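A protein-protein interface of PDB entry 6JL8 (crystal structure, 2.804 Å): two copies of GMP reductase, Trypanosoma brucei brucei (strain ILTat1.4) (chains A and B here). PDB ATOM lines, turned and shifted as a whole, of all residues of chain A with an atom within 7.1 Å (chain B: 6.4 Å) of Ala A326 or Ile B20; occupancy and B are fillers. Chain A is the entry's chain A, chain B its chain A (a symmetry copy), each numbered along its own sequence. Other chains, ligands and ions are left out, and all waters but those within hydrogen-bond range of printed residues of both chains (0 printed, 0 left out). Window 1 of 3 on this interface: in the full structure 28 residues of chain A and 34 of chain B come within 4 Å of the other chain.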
ATOM      1  N   VAL A 312       8.855 -12.589  -7.484  1.00  0.00           N
ATOM      2  CA  VAL A 312       9.901 -13.135  -8.342  1.00  0.00           C
ATOM      3  C   VAL A 312      10.344 -11.986  -9.229  1.00  0.00           C
ATOM      4  O   VAL A 312       9.632 -11.647 -10.183  1.00  0.00           O
ATOM      5  CB  VAL A 312       9.391 -14.303  -9.187  1.00  0.00           C
ATOM      6  CG1 VAL A 312      10.339 -14.598 -10.347  1.00  0.00           C
ATOM      7  CG2 VAL A 312       9.186 -15.551  -8.337  1.00  0.00           C
ATOM      8  N   GLY A 313      11.484 -11.340  -8.906  1.00  0.00           N
ATOM      9  CA  GLY A 313      12.005 -10.320  -9.802  1.00  0.00           C
ATOM     10  C   GLY A 313      12.229  -8.880  -9.325  1.00  0.00           C
ATOM     11  O   GLY A 313      13.268  -8.278  -9.636  1.00  0.00           O
ATOM     12  N   PRO A 314      11.270  -8.272  -8.610  1.00  0.00           N
ATOM     13  CA  PRO A 314      11.338  -6.812  -8.405  1.00  0.00           C
ATOM     14  C   PRO A 314      12.409  -6.362  -7.437  1.00  0.00           C
ATOM     15  O   PRO A 314      12.587  -5.146  -7.289  1.00  0.00           O
ATOM     16  CB  PRO A 314       9.955  -6.474  -7.854  1.00  0.00           C
ATOM     17  CG  PRO A 314       9.634  -7.681  -7.048  1.00  0.00           C
ATOM     18  CD  PRO A 314      10.101  -8.836  -7.913  1.00  0.00           C
ATOM     19  N   THR A 320      17.375 -11.444 -11.356  1.00  0.00           N
ATOM     20  CA  THR A 320      16.583 -12.487 -11.999  1.00  0.00           C
ATOM     21  C   THR A 320      16.177 -12.090 -13.405  1.00  0.00           C
ATOM     22  O   THR A 320      16.418 -12.837 -14.355  1.00  0.00           O
ATOM     23  CB  THR A 320      15.358 -12.775 -11.141  1.00  0.00           C
ATOM     24  OG1 THR A 320      15.804 -13.255  -9.868  1.00  0.00           O
ATOM     25  CG2 THR A 320      14.412 -13.830 -11.807  1.00  0.00           C
ATOM     26  N   ARG A 321      15.568 -10.899 -13.548  1.00  0.00           N
ATOM     27  CA  ARG A 321      15.049 -10.415 -14.831  1.00  0.00           C
ATOM     28  C   ARG A 321      16.086 -10.476 -15.932  1.00  0.00           C
ATOM     29  O   ARG A 321      15.816 -10.974 -17.026  1.00  0.00           O
ATOM     30  CB  ARG A 321      14.574  -8.973 -14.695  1.00  0.00           C
ATOM     31  CG  ARG A 321      13.523  -8.762 -13.613  1.00  0.00           C
ATOM     32  CD  ARG A 321      12.296  -8.206 -14.281  1.00  0.00           C
ATOM     33  NE  ARG A 321      11.362  -7.563 -13.380  1.00  0.00           N
ATOM     34  CZ  ARG A 321      10.803  -6.386 -13.630  1.00  0.00           C
ATOM     35  NH1 ARG A 321      11.084  -5.716 -14.739  1.00  0.00           N
ATOM     36  NH2 ARG A 321       9.943  -5.885 -12.776  1.00  0.00           N
ATOM     37  N   LEU A 322      17.288  -9.961 -15.673  1.00  0.00           N
ATOM     38  CA  LEU A 322      18.300  -9.966 -16.723  1.00  0.00           C
ATOM     39  C   LEU A 322      18.822 -11.369 -17.007  1.00  0.00           C
ATOM     40  O   LEU A 322      18.978 -11.750 -18.178  1.00  0.00           O
ATOM     41  CB  LEU A 322      19.437  -8.998 -16.374  1.00  0.00           C
ATOM     42  CG  LEU A 322      18.861  -7.609 -16.128  1.00  0.00           C
ATOM     43  CD1 LEU A 322      20.027  -6.660 -15.849  1.00  0.00           C
ATOM     44  CD2 LEU A 322      18.009  -7.128 -17.318  1.00  0.00           C
ATOM     45  N   VAL A 323      19.156 -12.128 -15.962  1.00  0.00           N
ATOM     46  CA  VAL A 323      19.764 -13.417 -16.240  1.00  0.00           C
ATOM     47  C   VAL A 323      18.745 -14.391 -16.814  1.00  0.00           C
ATOM     48  O   VAL A 323      19.045 -15.150 -17.746  1.00  0.00           O
ATOM     49  CB  VAL A 323      20.423 -13.964 -14.972  1.00  0.00           C
ATOM     50  CG1 VAL A 323      20.820 -15.412 -15.145  1.00  0.00           C
ATOM     51  CG2 VAL A 323      21.618 -13.111 -14.614  1.00  0.00           C
ATOM     52  N   ALA A 324      17.533 -14.405 -16.269  1.00  0.00           N
ATOM     53  CA  ALA A 324      16.584 -15.444 -16.630  1.00  0.00           C
ATOM     54  C   ALA A 324      15.414 -14.951 -17.459  1.00  0.00           C
ATOM     55  O   ALA A 324      14.818 -15.764 -18.177  1.00  0.00           O
ATOM     56  CB  ALA A 324      16.052 -16.142 -15.372  1.00  0.00           C
ATOM     57  N   GLY A 325      15.081 -13.658 -17.403  1.00  0.00           N
ATOM     58  CA  GLY A 325      13.949 -13.139 -18.158  1.00  0.00           C
ATOM     59  C   GLY A 325      12.614 -13.526 -17.574  1.00  0.00           C
ATOM     60  O   GLY A 325      11.608 -13.609 -18.290  1.00  0.00           O
ATOM     61  N   ALA A 326      12.572 -13.773 -16.277  1.00  0.00           N
ATOM     62  CA  ALA A 326      11.364 -14.238 -15.625  1.00  0.00           C
ATOM     63  C   ALA A 326      10.984 -13.260 -14.522  1.00  0.00           C
ATOM     64  O   ALA A 326      11.847 -12.563 -13.956  1.00  0.00           O
ATOM     65  CB  ALA A 326      11.561 -15.663 -15.051  1.00  0.00           C
ATOM     66  N   GLY A 327       9.689 -13.207 -14.243  1.00  0.00           N
ATOM     67  CA  GLY A 327       9.170 -12.378 -13.178  1.00  0.00           C
ATOM     68  C   GLY A 327       7.712 -12.057 -13.417  1.00  0.00           C
ATOM     69  O   GLY A 327       7.104 -12.510 -14.386  1.00  0.00           O
ATOM     70  N   VAL A 328       7.149 -11.294 -12.488  1.00  0.00           N
ATOM     71  CA  VAL A 328       5.807 -10.755 -12.643  1.00  0.00           C
ATOM     72  C   VAL A 328       5.845  -9.369 -12.017  1.00  0.00           C
ATOM     73  O   VAL A 328       6.370  -9.227 -10.911  1.00  0.00           O
ATOM     74  CB  VAL A 328       4.737 -11.649 -11.978  1.00  0.00           C
ATOM     75  CG1 VAL A 328       3.368 -11.006 -12.092  1.00  0.00           C
ATOM     76  CG2 VAL A 328       4.701 -13.037 -12.582  1.00  0.00           C
ATOM     77  N   VAL B  18       8.029  -8.091 -22.239  1.00  0.00           N
ATOM     78  CA  VAL B  18       7.554  -9.287 -21.578  1.00  0.00           C
ATOM     79  C   VAL B  18       8.541  -9.730 -20.519  1.00  0.00           C
ATOM     80  O   VAL B  18       9.726  -9.396 -20.559  1.00  0.00           O
ATOM     81  CB  VAL B  18       7.382 -10.404 -22.588  1.00  0.00           C
ATOM     82  CG1 VAL B  18       6.193 -10.078 -23.527  1.00  0.00           C
ATOM     83  CG2 VAL B  18       8.722 -10.557 -23.317  1.00  0.00           C
ATOM     84  N   LEU B  19       8.021 -10.496 -19.566  1.00  0.00           N
ATOM     85  CA  LEU B  19       8.791 -11.399 -18.725  1.00  0.00           C
ATOM     86  C   LEU B  19       8.107 -12.768 -18.738  1.00  0.00           C
ATOM     87  O   LEU B  19       6.897 -12.890 -19.025  1.00  0.00           O
ATOM     88  CB  LEU B  19       8.891 -10.884 -17.297  1.00  0.00           C
ATOM     89  CG  LEU B  19       9.330  -9.452 -17.102  1.00  0.00           C
ATOM     90  CD1 LEU B  19       8.817  -9.006 -15.756  1.00  0.00           C
ATOM     91  CD2 LEU B  19      10.876  -9.351 -17.173  1.00  0.00           C
ATOM     92  N   ILE B  20       8.901 -13.797 -18.428  1.00  0.00           N
ATOM     93  CA  ILE B  20       8.406 -15.165 -18.299  1.00  0.00           C
ATOM     94  C   ILE B  20       7.696 -15.296 -16.953  1.00  0.00           C
ATOM     95  O   ILE B  20       8.294 -15.054 -15.897  1.00  0.00           O
ATOM     96  CB  ILE B  20       9.565 -16.170 -18.415  1.00  0.00           C
ATOM     97  CG1 ILE B  20      10.023 -16.289 -19.860  1.00  0.00           C
ATOM     98  CG2 ILE B  20       9.194 -17.515 -17.904  1.00  0.00           C
ATOM     99  CD1 ILE B  20      11.509 -16.348 -20.000  1.00  0.00           C
ATOM    100  N   ILE B  21       6.418 -15.682 -16.981  1.00  0.00           N
ATOM    101  CA  ILE B  21       5.680 -15.944 -15.747  1.00  0.00           C
ATOM    102  C   ILE B  21       6.220 -17.227 -15.131  1.00  0.00           C
ATOM    103  O   ILE B  21       6.181 -18.263 -15.800  1.00  0.00           O
ATOM    104  CB  ILE B  21       4.176 -16.078 -16.008  1.00  0.00           C
ATOM    105  CG1 ILE B  21       3.604 -14.799 -16.621  1.00  0.00           C
ATOM    106  CG2 ILE B  21       3.462 -16.435 -14.717  1.00  0.00           C
ATOM    107  CD1 ILE B  21       2.272 -15.003 -17.237  1.00  0.00           C
ATOM    108  N   PRO B  22       6.742 -17.224 -13.896  1.00  0.00           N
ATOM    109  CA  PRO B  22       7.216 -18.483 -13.299  1.00  0.00           C
ATOM    110  C   PRO B  22       6.084 -19.494 -13.188  1.00  0.00           C
ATOM    111  O   PRO B  22       4.949 -19.140 -12.882  1.00  0.00           O
ATOM    112  CB  PRO B  22       7.719 -18.067 -11.912  1.00  0.00           C
ATOM    113  CG  PRO B  22       7.824 -16.618 -11.954  1.00  0.00           C
ATOM    114  CD  PRO B  22       6.880 -16.099 -12.957  1.00  0.00           C
ATOM    115  N   GLN B  23       6.419 -20.760 -13.438  1.00  0.00           N
ATOM    116  CA  GLN B  23       5.503 -21.891 -13.431  1.00  0.00           C
ATOM    117  C   GLN B  23       6.114 -22.973 -12.552  1.00  0.00           C
ATOM    118  O   GLN B  23       7.278 -22.872 -12.130  1.00  0.00           O
ATOM    119  CB  GLN B  23       5.251 -22.397 -14.851  1.00  0.00           C
ATOM    120  CG  GLN B  23       4.587 -21.375 -15.772  1.00  0.00           C
ATOM    121  CD  GLN B  23       3.482 -22.021 -16.569  1.00  0.00           C
ATOM    122  OE1 GLN B  23       3.752 -22.750 -17.540  1.00  0.00           O
ATOM    123  NE2 GLN B  23       2.221 -21.803 -16.148  1.00  0.00           N
ATOM    124  N   GLY B 358      18.556 -13.509 -20.450  1.00  0.00           N
ATOM    125  CA  GLY B 358      17.118 -13.510 -20.271  1.00  0.00           C
ATOM    126  C   GLY B 358      16.399 -13.219 -21.568  1.00  0.00           C
ATOM    127  O   GLY B 358      15.312 -13.748 -21.821  1.00  0.00           O
ATOM    128  N   SER B 361      16.323 -16.537 -23.131  1.00  0.00           N
ATOM    129  CA  SER B 361      15.203 -17.251 -22.528  1.00  0.00           C
ATOM    130  C   SER B 361      13.876 -16.874 -23.178  1.00  0.00           C
ATOM    131  O   SER B 361      13.035 -17.736 -23.437  1.00  0.00           O
ATOM    132  CB  SER B 361      15.126 -16.953 -21.031  1.00  0.00           C
ATOM    133  OG  SER B 361      16.096 -17.668 -20.327  1.00  0.00           O
ATOM    134  N   LYS B 362      13.656 -15.583 -23.405  1.00  0.00           N
ATOM    135  CA  LYS B 362      12.375 -15.160 -23.944  1.00  0.00           C
ATOM    136  C   LYS B 362      12.233 -15.617 -25.378  1.00  0.00           C
ATOM    137  O   LYS B 362      11.132 -15.990 -25.813  1.00  0.00           O
ATOM    138  CB  LYS B 362      12.236 -13.639 -23.841  1.00  0.00           C
ATOM    139  CG  LYS B 362      12.095 -13.122 -22.401  1.00  0.00           C
ATOM    140  CD  LYS B 362      12.240 -11.619 -22.380  1.00  0.00           C
ATOM    141  CE  LYS B 362      12.731 -11.119 -21.051  1.00  0.00           C
ATOM    142  NZ  LYS B 362      12.354  -9.708 -20.821  1.00  0.00           N
ATOM    143  N   GLY B 365      11.475 -19.306 -25.381  1.00  0.00           N
ATOM    144  CA  GLY B 365      10.144 -19.460 -24.825  1.00  0.00           C
ATOM    145  C   GLY B 365       9.071 -19.075 -25.817  1.00  0.00           C
ATOM    146  O   GLY B 365       8.016 -19.711 -25.884  1.00  0.00           O
ATOM    147  N   GLY B 454      16.345 -19.768 -16.997  1.00  0.00           N
ATOM    148  CA  GLY B 454      15.031 -19.332 -17.437  1.00  0.00           C
ATOM    149  C   GLY B 454      14.093 -20.498 -17.722  1.00  0.00           C
ATOM    150  O   GLY B 454      12.891 -20.435 -17.433  1.00  0.00           O
ATOM    151  N   MET B 455      14.632 -21.576 -18.291  1.00  0.00           N
ATOM    152  CA  MET B 455      13.852 -22.792 -18.459  1.00  0.00           C
ATOM    153  C   MET B 455      13.297 -23.282 -17.127  1.00  0.00           C
ATOM    154  O   MET B 455      12.164 -23.807 -17.061  1.00  0.00           O
ATOM    155  CB  MET B 455      14.716 -23.876 -19.124  1.00  0.00           C
ATOM    156  CG  MET B 455      15.341 -23.435 -20.440  1.00  0.00           C
ATOM    157  SD  MET B 455      16.549 -24.577 -21.124  1.00  0.00           S
ATOM    158  CE  MET B 455      15.574 -25.992 -21.546  1.00  0.00           C
ATOM    159  N   TYR B 457      12.349 -21.497 -14.648  1.00  0.00           N
ATOM    160  CA  TYR B 457      11.157 -20.727 -14.359  1.00  0.00           C
ATOM    161  C   TYR B 457       9.955 -21.230 -15.164  1.00  0.00           C
ATOM    162  O   TYR B 457       8.805 -21.188 -14.679  1.00  0.00           O
ATOM    163  CB  TYR B 457      11.436 -19.270 -14.626  1.00  0.00           C
ATOM    164  CG  TYR B 457      12.143 -18.642 -13.461  1.00  0.00           C
ATOM    165  CD1 TYR B 457      11.462 -18.373 -12.285  1.00  0.00           C
ATOM    166  CD2 TYR B 457      13.513 -18.351 -13.514  1.00  0.00           C
ATOM    167  CE1 TYR B 457      12.109 -17.832 -11.204  1.00  0.00           C
ATOM    168  CE2 TYR B 457      14.164 -17.790 -12.436  1.00  0.00           C
ATOM    169  CZ  TYR B 457      13.464 -17.544 -11.291  1.00  0.00           C
ATOM    170  OH  TYR B 457      14.101 -17.003 -10.227  1.00  0.00           O
ATOM    171  N   SER B 458      10.196 -21.723 -16.376  1.00  0.00           N
ATOM    172  CA  SER B 458       9.104 -22.231 -17.179  1.00  0.00           C
ATOM    173  C   SER B 458       8.748 -23.659 -16.819  1.00  0.00           C
ATOM    174  O   SER B 458       7.826 -24.225 -17.415  1.00  0.00           O
ATOM    175  CB  SER B 458       9.469 -22.128 -18.663  1.00  0.00           C
ATOM    176  OG  SER B 458       9.327 -20.799 -19.111  1.00  0.00           O
ATOM    177  N   MET B 466      10.558 -25.768 -22.977  1.00  0.00           N
ATOM    178  CA  MET B 466      10.600 -24.309 -22.906  1.00  0.00           C
ATOM    179  C   MET B 466       9.671 -23.680 -23.934  1.00  0.00           C
ATOM    180  O   MET B 466       9.009 -22.674 -23.659  1.00  0.00           O
ATOM    181  CB  MET B 466      12.027 -23.810 -23.136  1.00  0.00           C
ATOM    182  CG  MET B 466      12.210 -22.322 -22.913  1.00  0.00           C
ATOM    183  SD  MET B 466      11.662 -21.957 -21.246  1.00  0.00           S
ATOM    184  CE  MET B 466      12.434 -20.352 -20.935  1.00  0.00           C
ATOM    185  N   THR B 470       6.183 -22.058 -21.809  1.00  0.00           N
ATOM    186  CA  THR B 470       6.413 -20.695 -21.369  1.00  0.00           C
ATOM    187  C   THR B 470       5.145 -19.881 -21.533  1.00  0.00           C
ATOM    188  O   THR B 470       4.424 -20.027 -22.522  1.00  0.00           O
ATOM    189  CB  THR B 470       7.564 -20.067 -22.157  1.00  0.00           C
ATOM    190  OG1 THR B 470       8.800 -20.638 -21.712  1.00  0.00           O
ATOM    191  CG2 THR B 470       7.589 -18.556 -21.954  1.00  0.00           C
ATOM    192  N   ARG B 471       4.864 -19.060 -20.520  1.00  0.00           N
ATOM    193  CA  ARG B 471       3.794 -18.082 -20.502  1.00  0.00           C
ATOM    194  C   ARG B 471       4.412 -16.718 -20.241  1.00  0.00           C
ATOM    195  O   ARG B 471       5.264 -16.572 -19.347  1.00  0.00           O
ATOM    196  CB  ARG B 471       2.775 -18.395 -19.399  1.00  0.00           C
ATOM    197  CG  ARG B 471       1.929 -19.661 -19.611  1.00  0.00           C
ATOM    198  CD  ARG B 471       1.569 -19.795 -21.056  1.00  0.00           C
ATOM    199  NE  ARG B 471       0.596 -20.842 -21.327  1.00  0.00           N
ATOM    200  CZ  ARG B 471       0.866 -21.990 -21.956  1.00  0.00           C
ATOM    201  NH1 ARG B 471       2.103 -22.259 -22.372  1.00  0.00           N
ATOM    202  NH2 ARG B 471      -0.115 -22.872 -22.171  1.00  0.00           N
ATOM    203  N   PHE B 472       3.959 -15.718 -20.993  1.00  0.00           N
ATOM    204  CA  PHE B 472       4.458 -14.352 -20.903  1.00  0.00           C
ATOM    205  C   PHE B 472       3.465 -13.420 -20.210  1.00  0.00           C
ATOM    206  O   PHE B 472       2.245 -13.609 -20.281  1.00  0.00           O
ATOM    207  CB  PHE B 472       4.731 -13.790 -22.295  1.00  0.00           C
ATOM    208  CG  PHE B 472       5.840 -14.453 -23.016  1.00  0.00           C
ATOM    209  CD1 PHE B 472       7.164 -14.264 -22.597  1.00  0.00           C
ATOM    210  CD2 PHE B 472       5.574 -15.246 -24.147  1.00  0.00           C
ATOM    211  CE1 PHE B 472       8.214 -14.886 -23.268  1.00  0.00           C
ATOM    212  CE2 PHE B 472       6.617 -15.858 -24.835  1.00  0.00           C
ATOM    213  CZ  PHE B 472       7.960 -15.656 -24.399  1.00  0.00           C
ATOM    214  N   VAL B 473       4.005 -12.370 -19.597  1.00  0.00           N
ATOM    215  CA  VAL B 473       3.240 -11.260 -19.043  1.00  0.00           C
ATOM    216  C   VAL B 473       3.872  -9.971 -19.558  1.00  0.00           C
ATOM    217  O   VAL B 473       5.094  -9.882 -19.700  1.00  0.00           O
ATOM    218  CB  VAL B 473       3.221 -11.285 -17.497  1.00  0.00           C
ATOM    219  CG1 VAL B 473       4.633 -11.376 -16.974  1.00  0.00           C
ATOM    220  CG2 VAL B 473       2.617 -10.027 -16.956  1.00  0.00           C
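O of Val A323 sits at hydrogen-bond distance from N of Gly B358 (3.2 Å). The backbone carbonyl oxygen (O) of Gly A325 sits at hydrogen-bond distance from the backbone NH (N) of Ile B20, 2.7 Å away. The backbone carbonyl oxygen (O) of Ala A324 lies close to the side-chain hydroxyl (OG) of Ser B361 (3.1 Å). The backbone carbonyl oxygen of Ile B20 sits at hydrogen-bond distance from the backbone NH of Gly A327 (2.8 Å). O of Leu A322 is in hydrogen-bond range of N of Gly B358 (2.9 Å).
Among the printed residues, pairs that only touch across the chains: Ala A326 with Ile B20 (3.2 Å), Arg A321 with Leu B19 (3.4 Å), Ala A326 with Tyr B457 (3.4 Å), Gly A325 with Gly B358 (3.5 Å), Thr A320 with Tyr B457 (3.6 Å), Ala A324 with Gly B358 (3.6 Å), Val A312 with Pro B22 (3.6 Å), Gly A325 with Leu B19 (3.6 Å), Ala A324 with Gly B454 (3.7 Å), Gly A325 with Lys B362 (3.7 Å), Gly A327 with Val B473 (3.8 Å), Val A328 with Pro B22 (3.8 Å), Gly A327 with Leu B19 (3.8 Å), Val A312 with Tyr B457 (3.8 Å), Ala A324 with Ile B20 (3.8 Å), Ala A324 with Tyr B457 (3.8 Å), Gly A327 with Pro B22 (3.9 Å) and Gly A327 with Ile B21 (3.96 Å).
The backbone carbonyl oxygen of Val A312 is in hydrogen-bond range of the backbone NH of Val A328, 3.4 Å away. O of Val B473 is in hydrogen-bond range of N of Leu B19, at 3.0 Å. O of Thr A320 lies within hydrogen-bond range of N of Gly A325 (3.4 Å). The backbone NH of Gln B23 is in hydrogen-bond range of the backbone carbonyl oxygen of Tyr B457, at 2.7 Å. The backbone carbonyl oxygen (O) of Arg B471 lies within hydrogen-bond range of the backbone NH (N) of Ile B21 (2.8 Å). NZ of Lys B362 lies within hydrogen-bond range of O of Val B18, at 2.7 Å.
Of the 19 printed residues of chain B, 10 touch a printed residue of chain A. Printed residues of chain A that touch a printed residue of chain B: Val A312, Thr A320, Arg A321, Leu A322, Val A323, Ala A324, Gly A325, Ala A326, Gly A327 and Val A328. Hydrophobic or aromatic side chains of chain A within 4 Å of the printed part of chain B: Val A312, Ala A324, Ala A326 and Val A328. Along chain A the printed residues that touch a printed residue of chain B span positions 312 to 328. Among the printed residues, 23 pairs touch across the chains.
Printed residues of chain B within 4 Å of Arg A321: Leu B19. Printed residues of chain B within 4 Å of Ala A324: Ile B20, Gly B358, Ser B361, Gly B454 and Tyr B457. Of chain B, only Ile B20 (3.2 Å) and Tyr B457 (3.4 Å) come within 4 Å of Ala A326. Ile B20 touches four residues of chain A. Printed residues of chain A within 4 Å of Ile B21: Gly A327. Printed residues of chain A within 4 Å of Lys B362: Gly A325. Of the printed residues of chain A, Val B473 touches Gly A327. The nearest printed residue of chain B that does not touch Val A312 is Ile B20 (5.9 Å).
No position is printed for both chains.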
